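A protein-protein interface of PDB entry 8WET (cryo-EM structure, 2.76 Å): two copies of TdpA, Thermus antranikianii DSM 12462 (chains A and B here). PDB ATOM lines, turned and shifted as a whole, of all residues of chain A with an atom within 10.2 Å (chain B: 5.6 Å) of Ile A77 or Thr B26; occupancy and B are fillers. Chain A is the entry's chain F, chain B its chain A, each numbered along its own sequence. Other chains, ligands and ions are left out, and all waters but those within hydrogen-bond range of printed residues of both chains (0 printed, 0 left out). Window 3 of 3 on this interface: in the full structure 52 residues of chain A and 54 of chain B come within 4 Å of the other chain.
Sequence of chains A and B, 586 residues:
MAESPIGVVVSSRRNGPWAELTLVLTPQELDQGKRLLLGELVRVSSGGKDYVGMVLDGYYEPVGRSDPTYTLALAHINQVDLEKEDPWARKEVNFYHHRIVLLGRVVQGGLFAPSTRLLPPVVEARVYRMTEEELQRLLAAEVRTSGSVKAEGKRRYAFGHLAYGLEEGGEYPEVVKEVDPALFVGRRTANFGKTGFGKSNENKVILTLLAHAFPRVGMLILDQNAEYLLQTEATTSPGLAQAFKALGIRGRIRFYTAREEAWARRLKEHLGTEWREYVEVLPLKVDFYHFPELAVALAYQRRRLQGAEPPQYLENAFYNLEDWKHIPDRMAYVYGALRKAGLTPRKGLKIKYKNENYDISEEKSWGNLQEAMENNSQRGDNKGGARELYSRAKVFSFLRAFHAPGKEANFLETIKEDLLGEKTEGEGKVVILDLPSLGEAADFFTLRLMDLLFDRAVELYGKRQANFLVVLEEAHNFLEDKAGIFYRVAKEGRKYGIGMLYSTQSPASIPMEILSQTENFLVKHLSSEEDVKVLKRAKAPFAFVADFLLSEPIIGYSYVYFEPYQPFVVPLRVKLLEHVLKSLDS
O of Ile A77 sits close to OE1 of Gln B28, 3.3 Å away. A ring nitrogen (NE2) of His A76 sits at hydrogen-bond distance from the side-chain carboxylate (OE2) of Glu B29, at 2.6 Å.
Leu A72 touches Val B8. CD2 of His A76 touches CG2 of Thr B26, at 3.6 Å. His A76 touches Gln B28 (O to NE2, 3.7 Å). Thr B26 touches Ile A77 (CG2 to CG1, 3.7 Å).
Printed residues of chain B within 4 Å of Leu A72: Val B8. Of the printed residues of chain B, His A76 touches Thr B26 (3.6 Å), Gln B28 (3.7 Å) and Glu B29 (2.6 Å). Of chain B, only Thr B26 (3.7 Å) and Gln B28 (3.3 Å) come within 4 Å of Ile A77. Printed residues of chain A within 4 Å of Val B8: Leu A72. No residue of chain A comes within 4 Å of Leu B25. Printed residues of chain A within 4 Å of Thr B26: His A76 and Ile A77. No residue of chain A comes within 4 Å of Pro B27. Gln B28 touches two residues of chain A. Glu B29 touches just one residue of chain A: His A76.
O of Val B8 sits at hydrogen-bond distance from N of Val B24, 3.0 Å away. The side-chain hydroxyl (OG1) of Thr B26 sits close to the side-chain carboxylate (OE2) of Glu B29 (3.0 Å).
Printed residues of chain A that touch a printed residue of chain B: Leu A72, His A76 and Ile A77. Hydrophobic or aromatic side chains of chain A that line the printed part of chain B: Leu A72, His A76 and Ile A77. Along chain A the printed residues that touch a printed residue of chain B span positions 72 to 77. Hydrophobic or aromatic side chains of chain B within 4 Å of the printed part of chain A: Val B8. Among the printed residues, 6 pairs touch across the chains. Among the printed residues, no Asp or Glu carboxylate lies within 4 Å of a Lys or Arg side-chain nitrogen of the other chain.
No position is printed for both chains.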
ATOM      1  N   THR A  69      23.643 -11.756 -17.098  1.00  0.00           N
ATOM      2  CA  THR A  69      23.761 -12.278 -18.455  1.00  0.00           C
ATOM      3  C   THR A  69      22.396 -12.382 -19.123  1.00  0.00           C
ATOM      4  O   THR A  69      22.214 -11.931 -20.258  1.00  0.00           O
ATOM      5  CB  THR A  69      24.457 -13.640 -18.436  1.00  0.00           C
ATOM      6  OG1 THR A  69      25.756 -13.506 -17.849  1.00  0.00           O
ATOM      7  CG2 THR A  69      24.602 -14.182 -19.848  1.00  0.00           C
ATOM      8  N   TYR A  70      21.420 -12.960 -18.422  1.00  0.00           N
ATOM      9  CA  TYR A  70      20.079 -13.103 -18.982  1.00  0.00           C
ATOM     10  C   TYR A  70      19.440 -11.746 -19.250  1.00  0.00           C
ATOM     11  O   TYR A  70      18.850 -11.527 -20.315  1.00  0.00           O
ATOM     12  CB  TYR A  70      19.212 -13.930 -18.032  1.00  0.00           C
ATOM     13  CG  TYR A  70      17.856 -14.305 -18.583  1.00  0.00           C
ATOM     14  CD1 TYR A  70      17.705 -15.393 -19.430  1.00  0.00           C
ATOM     15  CD2 TYR A  70      16.723 -13.578 -18.244  1.00  0.00           C
ATOM     16  CE1 TYR A  70      16.467 -15.743 -19.929  1.00  0.00           C
ATOM     17  CE2 TYR A  70      15.482 -13.919 -18.739  1.00  0.00           C
ATOM     18  CZ  TYR A  70      15.359 -15.002 -19.582  1.00  0.00           C
ATOM     19  OH  TYR A  70      14.124 -15.345 -20.078  1.00  0.00           O
ATOM     20  N   THR A  71      19.553 -10.820 -18.296  1.00  0.00           N
ATOM     21  CA  THR A  71      18.942  -9.505 -18.457  1.00  0.00           C
ATOM     22  C   THR A  71      19.547  -8.760 -19.640  1.00  0.00           C
ATOM     23  O   THR A  71      18.822  -8.221 -20.485  1.00  0.00           O
ATOM     24  CB  THR A  71      19.101  -8.693 -17.172  1.00  0.00           C
ATOM     25  OG1 THR A  71      18.383  -9.334 -16.110  1.00  0.00           O
ATOM     26  CG2 THR A  71      18.566  -7.284 -17.360  1.00  0.00           C
ATOM     27  N   LEU A  72      20.879  -8.731 -19.725  1.00  0.00           N
ATOM     28  CA  LEU A  72      21.531  -8.036 -20.829  1.00  0.00           C
ATOM     29  C   LEU A  72      21.234  -8.708 -22.165  1.00  0.00           C
ATOM     30  O   LEU A  72      21.024  -8.023 -23.172  1.00  0.00           O
ATOM     31  CB  LEU A  72      23.037  -7.953 -20.582  1.00  0.00           C
ATOM     32  CG  LEU A  72      23.464  -7.072 -19.405  1.00  0.00           C
ATOM     33  CD1 LEU A  72      24.905  -7.348 -19.011  1.00  0.00           C
ATOM     34  CD2 LEU A  72      23.268  -5.600 -19.729  1.00  0.00           C
ATOM     35  N   ALA A  73      21.203 -10.043 -22.196  1.00  0.00           N
ATOM     36  CA  ALA A  73      20.927 -10.745 -23.445  1.00  0.00           C
ATOM     37  C   ALA A  73      19.516 -10.465 -23.945  1.00  0.00           C
ATOM     38  O   ALA A  73      19.318 -10.208 -25.138  1.00  0.00           O
ATOM     39  CB  ALA A  73      21.145 -12.246 -23.261  1.00  0.00           C
ATOM     40  N   LEU A  74      18.522 -10.506 -23.054  1.00  0.00           N
ATOM     41  CA  LEU A  74      17.159 -10.211 -23.489  1.00  0.00           C
ATOM     42  C   LEU A  74      16.967  -8.736 -23.811  1.00  0.00           C
ATOM     43  O   LEU A  74      16.139  -8.398 -24.664  1.00  0.00           O
ATOM     44  CB  LEU A  74      16.143 -10.670 -22.443  1.00  0.00           C
ATOM     45  CG  LEU A  74      15.706 -12.134 -22.555  1.00  0.00           C
ATOM     46  CD1 LEU A  74      16.807 -13.104 -22.157  1.00  0.00           C
ATOM     47  CD2 LEU A  74      14.446 -12.373 -21.735  1.00  0.00           C
ATOM     48  N   ALA A  75      17.704  -7.843 -23.148  1.00  0.00           N
ATOM     49  CA  ALA A  75      17.665  -6.442 -23.544  1.00  0.00           C
ATOM     50  C   ALA A  75      18.223  -6.258 -24.948  1.00  0.00           C
ATOM     51  O   ALA A  75      17.664  -5.505 -25.753  1.00  0.00           O
ATOM     52  CB  ALA A  75      18.438  -5.589 -22.539  1.00  0.00           C
ATOM     53  N   HIS A  76      19.320  -6.948 -25.265  1.00  0.00           N
ATOM     54  CA  HIS A  76      19.930  -6.817 -26.585  1.00  0.00           C
ATOM     55  C   HIS A  76      19.064  -7.450 -27.669  1.00  0.00           C
ATOM     56  O   HIS A  76      18.998  -6.939 -28.793  1.00  0.00           O
ATOM     57  CB  HIS A  76      21.323  -7.446 -26.577  1.00  0.00           C
ATOM     58  CG  HIS A  76      22.009  -7.419 -27.907  1.00  0.00           C
ATOM     59  ND1 HIS A  76      22.304  -6.247 -28.568  1.00  0.00           N
ATOM     60  CD2 HIS A  76      22.460  -8.422 -28.697  1.00  0.00           C
ATOM     61  CE1 HIS A  76      22.907  -6.529 -29.710  1.00  0.00           C
ATOM     62  NE2 HIS A  76      23.013  -7.841 -29.812  1.00  0.00           N
ATOM     63  N   ILE A  77      18.401  -8.565 -27.353  1.00  0.00           N
ATOM     64  CA  ILE A  77      17.606  -9.274 -28.354  1.00  0.00           C
ATOM     65  C   ILE A  77      16.450  -8.407 -28.839  1.00  0.00           C
ATOM     66  O   ILE A  77      16.157  -8.351 -30.039  1.00  0.00           O
ATOM     67  CB  ILE A  77      17.109 -10.616 -27.785  1.00  0.00           C
ATOM     68  CG1 ILE A  77      18.229 -11.657 -27.822  1.00  0.00           C
ATOM     69  CG2 ILE A  77      15.898 -11.116 -28.554  1.00  0.00           C
ATOM     70  CD1 ILE A  77      17.921 -12.913 -27.041  1.00  0.00           C
ATOM     71  N   ASN A  78      15.786  -7.704 -27.919  1.00  0.00           N
ATOM     72  CA  ASN A  78      14.609  -6.904 -28.236  1.00  0.00           C
ATOM     73  C   ASN A  78      14.948  -5.448 -28.534  1.00  0.00           C
ATOM     74  O   ASN A  78      14.129  -4.563 -28.255  1.00  0.00           O
ATOM     75  CB  ASN A  78      13.600  -6.983 -27.089  1.00  0.00           C
ATOM     76  CG  ASN A  78      13.085  -8.389 -26.862  1.00  0.00           C
ATOM     77  OD1 ASN A  78      12.845  -9.135 -27.809  1.00  0.00           O
ATOM     78  ND2 ASN A  78      12.913  -8.758 -25.599  1.00  0.00           N
ATOM     79  N   GLN A  79      16.124  -5.183 -29.107  1.00  0.00           N
ATOM     80  CA  GLN A  79      16.648  -3.833 -29.305  1.00  0.00           C
ATOM     81  C   GLN A  79      16.883  -3.167 -27.955  1.00  0.00           C
ATOM     82  O   GLN A  79      17.930  -3.381 -27.337  1.00  0.00           O
ATOM     83  CB  GLN A  79      15.715  -2.985 -30.177  1.00  0.00           C
ATOM     84  CG  GLN A  79      15.227  -3.673 -31.447  1.00  0.00           C
ATOM     85  CD  GLN A  79      16.323  -4.435 -32.167  1.00  0.00           C
ATOM     86  OE1 GLN A  79      17.388  -3.891 -32.458  1.00  0.00           O
ATOM     87  NE2 GLN A  79      16.064  -5.704 -32.460  1.00  0.00           N
ATOM     88  N   VAL A  80      15.930  -2.349 -27.503  1.00  0.00           N
ATOM     89  CA  VAL A  80      15.924  -1.760 -26.164  1.00  0.00           C
ATOM     90  C   VAL A  80      17.209  -0.997 -25.864  1.00  0.00           C
ATOM     91  O   VAL A  80      18.203  -1.581 -25.417  1.00  0.00           O
ATOM     92  CB  VAL A  80      15.682  -2.834 -25.085  1.00  0.00           C
ATOM     93  CG1 VAL A  80      15.641  -2.198 -23.703  1.00  0.00           C
ATOM     94  CG2 VAL A  80      14.393  -3.578 -25.352  1.00  0.00           C
ATOM     95  N   ASP A  81      17.198   0.312 -26.090  1.00  0.00           N
ATOM     96  CA  ASP A  81      18.290   1.163 -25.626  1.00  0.00           C
ATOM     97  C   ASP A  81      18.164   1.298 -24.115  1.00  0.00           C
ATOM     98  O   ASP A  81      17.354   2.080 -23.614  1.00  0.00           O
ATOM     99  CB  ASP A  81      18.246   2.522 -26.315  1.00  0.00           C
ATOM    100  CG  ASP A  81      19.477   3.357 -26.031  1.00  0.00           C
ATOM    101  OD1 ASP A  81      20.469   2.800 -25.517  1.00  0.00           O
ATOM    102  OD2 ASP A  81      19.455   4.571 -26.326  1.00  0.00           O
ATOM    103  N   LEU A  82      18.978   0.536 -23.380  1.00  0.00           N
ATOM    104  CA  LEU A  82      18.784   0.384 -21.941  1.00  0.00           C
ATOM    105  C   LEU A  82      18.877   1.702 -21.183  1.00  0.00           C
ATOM    106  O   LEU A  82      18.275   1.827 -20.112  1.00  0.00           O
ATOM    107  CB  LEU A  82      19.807  -0.603 -21.376  1.00  0.00           C
ATOM    108  CG  LEU A  82      19.416  -2.081 -21.405  1.00  0.00           C
ATOM    109  CD1 LEU A  82      20.494  -2.930 -20.754  1.00  0.00           C
ATOM    110  CD2 LEU A  82      18.079  -2.294 -20.722  1.00  0.00           C
ATOM    111  N   VAL B   8      26.797  -8.676 -27.033  1.00  0.00           N
ATOM    112  CA  VAL B   8      26.547  -7.950 -25.795  1.00  0.00           C
ATOM    113  C   VAL B   8      27.590  -8.373 -24.768  1.00  0.00           C
ATOM    114  O   VAL B   8      27.869  -9.565 -24.604  1.00  0.00           O
ATOM    115  CB  VAL B   8      25.109  -8.182 -25.276  1.00  0.00           C
ATOM    116  CG1 VAL B   8      24.815  -9.666 -25.118  1.00  0.00           C
ATOM    117  CG2 VAL B   8      24.886  -7.445 -23.966  1.00  0.00           C
ATOM    118  N   VAL B  24      28.643 -12.300 -25.555  1.00  0.00           N
ATOM    119  CA  VAL B  24      27.639 -13.310 -25.866  1.00  0.00           C
ATOM    120  C   VAL B  24      27.029 -12.985 -27.222  1.00  0.00           C
ATOM    121  O   VAL B  24      26.649 -11.837 -27.477  1.00  0.00           O
ATOM    122  CB  VAL B  24      26.549 -13.381 -24.781  1.00  0.00           C
ATOM    123  CG1 VAL B  24      25.526 -14.448 -25.121  1.00  0.00           C
ATOM    124  CG2 VAL B  24      27.169 -13.654 -23.425  1.00  0.00           C
ATOM    125  N   LEU B  25      26.942 -13.990 -28.088  1.00  0.00           N
ATOM    126  CA  LEU B  25      26.296 -13.858 -29.388  1.00  0.00           C
ATOM    127  C   LEU B  25      24.871 -14.389 -29.285  1.00  0.00           C
ATOM    128  O   LEU B  25      24.660 -15.538 -28.884  1.00  0.00           O
ATOM    129  CB  LEU B  25      27.078 -14.607 -30.467  1.00  0.00           C
ATOM    130  CG  LEU B  25      28.478 -14.083 -30.787  1.00  0.00           C
ATOM    131  CD1 LEU B  25      29.236 -15.073 -31.650  1.00  0.00           C
ATOM    132  CD2 LEU B  25      28.404 -12.732 -31.469  1.00  0.00           C
ATOM    133  N   THR B  26      23.903 -13.554 -29.645  1.00  0.00           N
ATOM    134  CA  THR B  26      22.495 -13.881 -29.499  1.00  0.00           C
ATOM    135  C   THR B  26      21.997 -14.697 -30.690  1.00  0.00           C
ATOM    136  O   THR B  26      22.654 -14.754 -31.733  1.00  0.00           O
ATOM    137  CB  THR B  26      21.680 -12.599 -29.348  1.00  0.00           C
ATOM    138  OG1 THR B  26      22.024 -11.683 -30.393  1.00  0.00           O
ATOM    139  CG2 THR B  26      21.960 -11.954 -28.001  1.00  0.00           C
ATOM    140  N   PRO B  27      20.842 -15.362 -30.553  1.00  0.00           N
ATOM    141  CA  PRO B  27      20.311 -16.140 -31.686  1.00  0.00           C
ATOM    142  C   PRO B  27      20.089 -15.325 -32.947  1.00  0.00           C
ATOM    143  O   PRO B  27      20.296 -15.846 -34.050  1.00  0.00           O
ATOM    144  CB  PRO B  27      18.988 -16.690 -31.138  1.00  0.00           C
ATOM    145  CG  PRO B  27      19.188 -16.755 -29.677  1.00  0.00           C
ATOM    146  CD  PRO B  27      20.072 -15.598 -29.318  1.00  0.00           C
ATOM    147  N   GLN B  28      19.677 -14.062 -32.825  1.00  0.00           N
ATOM    148  CA  GLN B  28      19.438 -13.232 -34.000  1.00  0.00           C
ATOM    149  C   GLN B  28      20.705 -12.958 -34.798  1.00  0.00           C
ATOM    150  O   GLN B  28      20.607 -12.520 -35.949  1.00  0.00           O
ATOM    151  CB  GLN B  28      18.799 -11.906 -33.587  1.00  0.00           C
ATOM    152  CG  GLN B  28      19.758 -10.942 -32.906  1.00  0.00           C
ATOM    153  CD  GLN B  28      19.077  -9.667 -32.449  1.00  0.00           C
ATOM    154  OE1 GLN B  28      17.863  -9.517 -32.581  1.00  0.00           O
ATOM    155  NE2 GLN B  28      19.859  -8.738 -31.911  1.00  0.00           N
ATOM    156  N   GLU B  29      21.880 -13.201 -34.222  1.00  0.00           N
ATOM    157  CA  GLU B  29      23.146 -12.954 -34.895  1.00  0.00           C
ATOM    158  C   GLU B  29      23.793 -14.219 -35.436  1.00  0.00           C
ATOM    159  O   GLU B  29      24.475 -14.159 -36.464  1.00  0.00           O
ATOM    160  CB  GLU B  29      24.117 -12.258 -33.940  1.00  0.00           C
ATOM    161  CG  GLU B  29      23.536 -11.012 -33.305  1.00  0.00           C
ATOM    162  CD  GLU B  29      24.296 -10.582 -32.075  1.00  0.00           C
ATOM    163  OE1 GLU B  29      25.272 -11.270 -31.712  1.00  0.00           O
ATOM    164  OE2 GLU B  29      23.918  -9.559 -31.469  1.00  0.00           O
ATOM    165  N   LEU B  30      23.601 -15.359 -34.771  1.00  0.00           N
ATOM    166  CA  LEU B  30      24.097 -16.618 -35.312  1.00  0.00           C
ATOM    167  C   LEU B  30      23.277 -17.086 -36.505  1.00  0.00           C
ATOM    168  O   LEU B  30      23.770 -17.890 -37.303  1.00  0.00           O
ATOM    169  CB  LEU B  30      24.111 -17.693 -34.226  1.00  0.00           C
ATOM    170  CG  LEU B  30      24.875 -17.343 -32.948  1.00  0.00           C
ATOM    171  CD1 LEU B  30      24.524 -18.306 -31.827  1.00  0.00           C
ATOM    172  CD2 LEU B  30      26.373 -17.338 -33.205  1.00  0.00           C
ATOM    173  N   ASP B  31      22.040 -16.606 -36.641  1.00  0.00           N
ATOM    174  CA  ASP B  31      21.247 -16.904 -37.826  1.00  0.00           C
ATOM    175  C   ASP B  31      21.700 -16.092 -39.031  1.00  0.00           C
ATOM    176  O   ASP B  31      21.519 -16.527 -40.172  1.00  0.00           O
ATOM    177  CB  ASP B  31      19.765 -16.645 -37.547  1.00  0.00           C
ATOM    178  CG  ASP B  31      19.209 -17.550 -36.465  1.00  0.00           C
ATOM    179  OD1 ASP B  31      19.934 -18.463 -36.020  1.00  0.00           O
ATOM    180  OD2 ASP B  31      18.045 -17.347 -36.060  1.00  0.00           O
ATOM    181  N   LYS B  91      15.285 -20.418 -29.767  1.00  0.00           N
ATOM    182  CA  LYS B  91      15.765 -19.100 -29.373  1.00  0.00           C
ATOM    183  C   LYS B  91      16.377 -19.082 -27.980  1.00  0.00           C
ATOM    184  O   LYS B  91      17.058 -18.110 -27.632  1.00  0.00           O
ATOM    185  CB  LYS B  91      14.625 -18.082 -29.433  1.00  0.00           C
ATOM    186  CG  LYS B  91      14.088 -17.825 -30.827  1.00  0.00           C
ATOM    187  CD  LYS B  91      14.982 -16.870 -31.599  1.00  0.00           C
ATOM    188  CE  LYS B  91      14.658 -15.421 -31.275  1.00  0.00           C
ATOM    189  NZ  LYS B  91      15.384 -14.478 -32.169  1.00  0.00           N
ATOM    190  N   ASN B  94      20.413 -20.982 -28.522  1.00  0.00           N
ATOM    191  CA  ASN B  94      21.333 -20.596 -29.591  1.00  0.00           C
ATOM    192  C   ASN B  94      22.176 -19.399 -29.150  1.00  0.00           C
ATOM    193  O   ASN B  94      21.997 -18.267 -29.597  1.00  0.00           O
ATOM    194  CB  ASN B  94      20.557 -20.299 -30.870  1.00  0.00           C
ATOM    195  CG  ASN B  94      21.345 -20.625 -32.122  1.00  0.00           C
ATOM    196  OD1 ASN B  94      22.239 -21.470 -32.104  1.00  0.00           O
ATOM    197  ND2 ASN B  94      21.015 -19.956 -33.219  1.00  0.00           N
ATOM    198  N   PHE B  95      23.125 -19.677 -28.260  1.00  0.00           N
ATOM    199  CA  PHE B  95      24.035 -18.667 -27.744  1.00  0.00           C
ATOM    200  C   PHE B  95      25.471 -19.157 -27.876  1.00  0.00           C
ATOM    201  O   PHE B  95      25.726 -20.347 -28.073  1.00  0.00           O
ATOM    202  CB  PHE B  95      23.736 -18.332 -26.276  1.00  0.00           C
ATOM    203  CG  PHE B  95      22.437 -17.610 -26.068  1.00  0.00           C
ATOM    204  CD1 PHE B  95      22.381 -16.229 -26.129  1.00  0.00           C
ATOM    205  CD2 PHE B  95      21.275 -18.311 -25.803  1.00  0.00           C
ATOM    206  CE1 PHE B  95      21.189 -15.563 -25.935  1.00  0.00           C
ATOM    207  CE2 PHE B  95      20.081 -17.649 -25.608  1.00  0.00           C
ATOM    208  CZ  PHE B  95      20.039 -16.273 -25.674  1.00  0.00           C
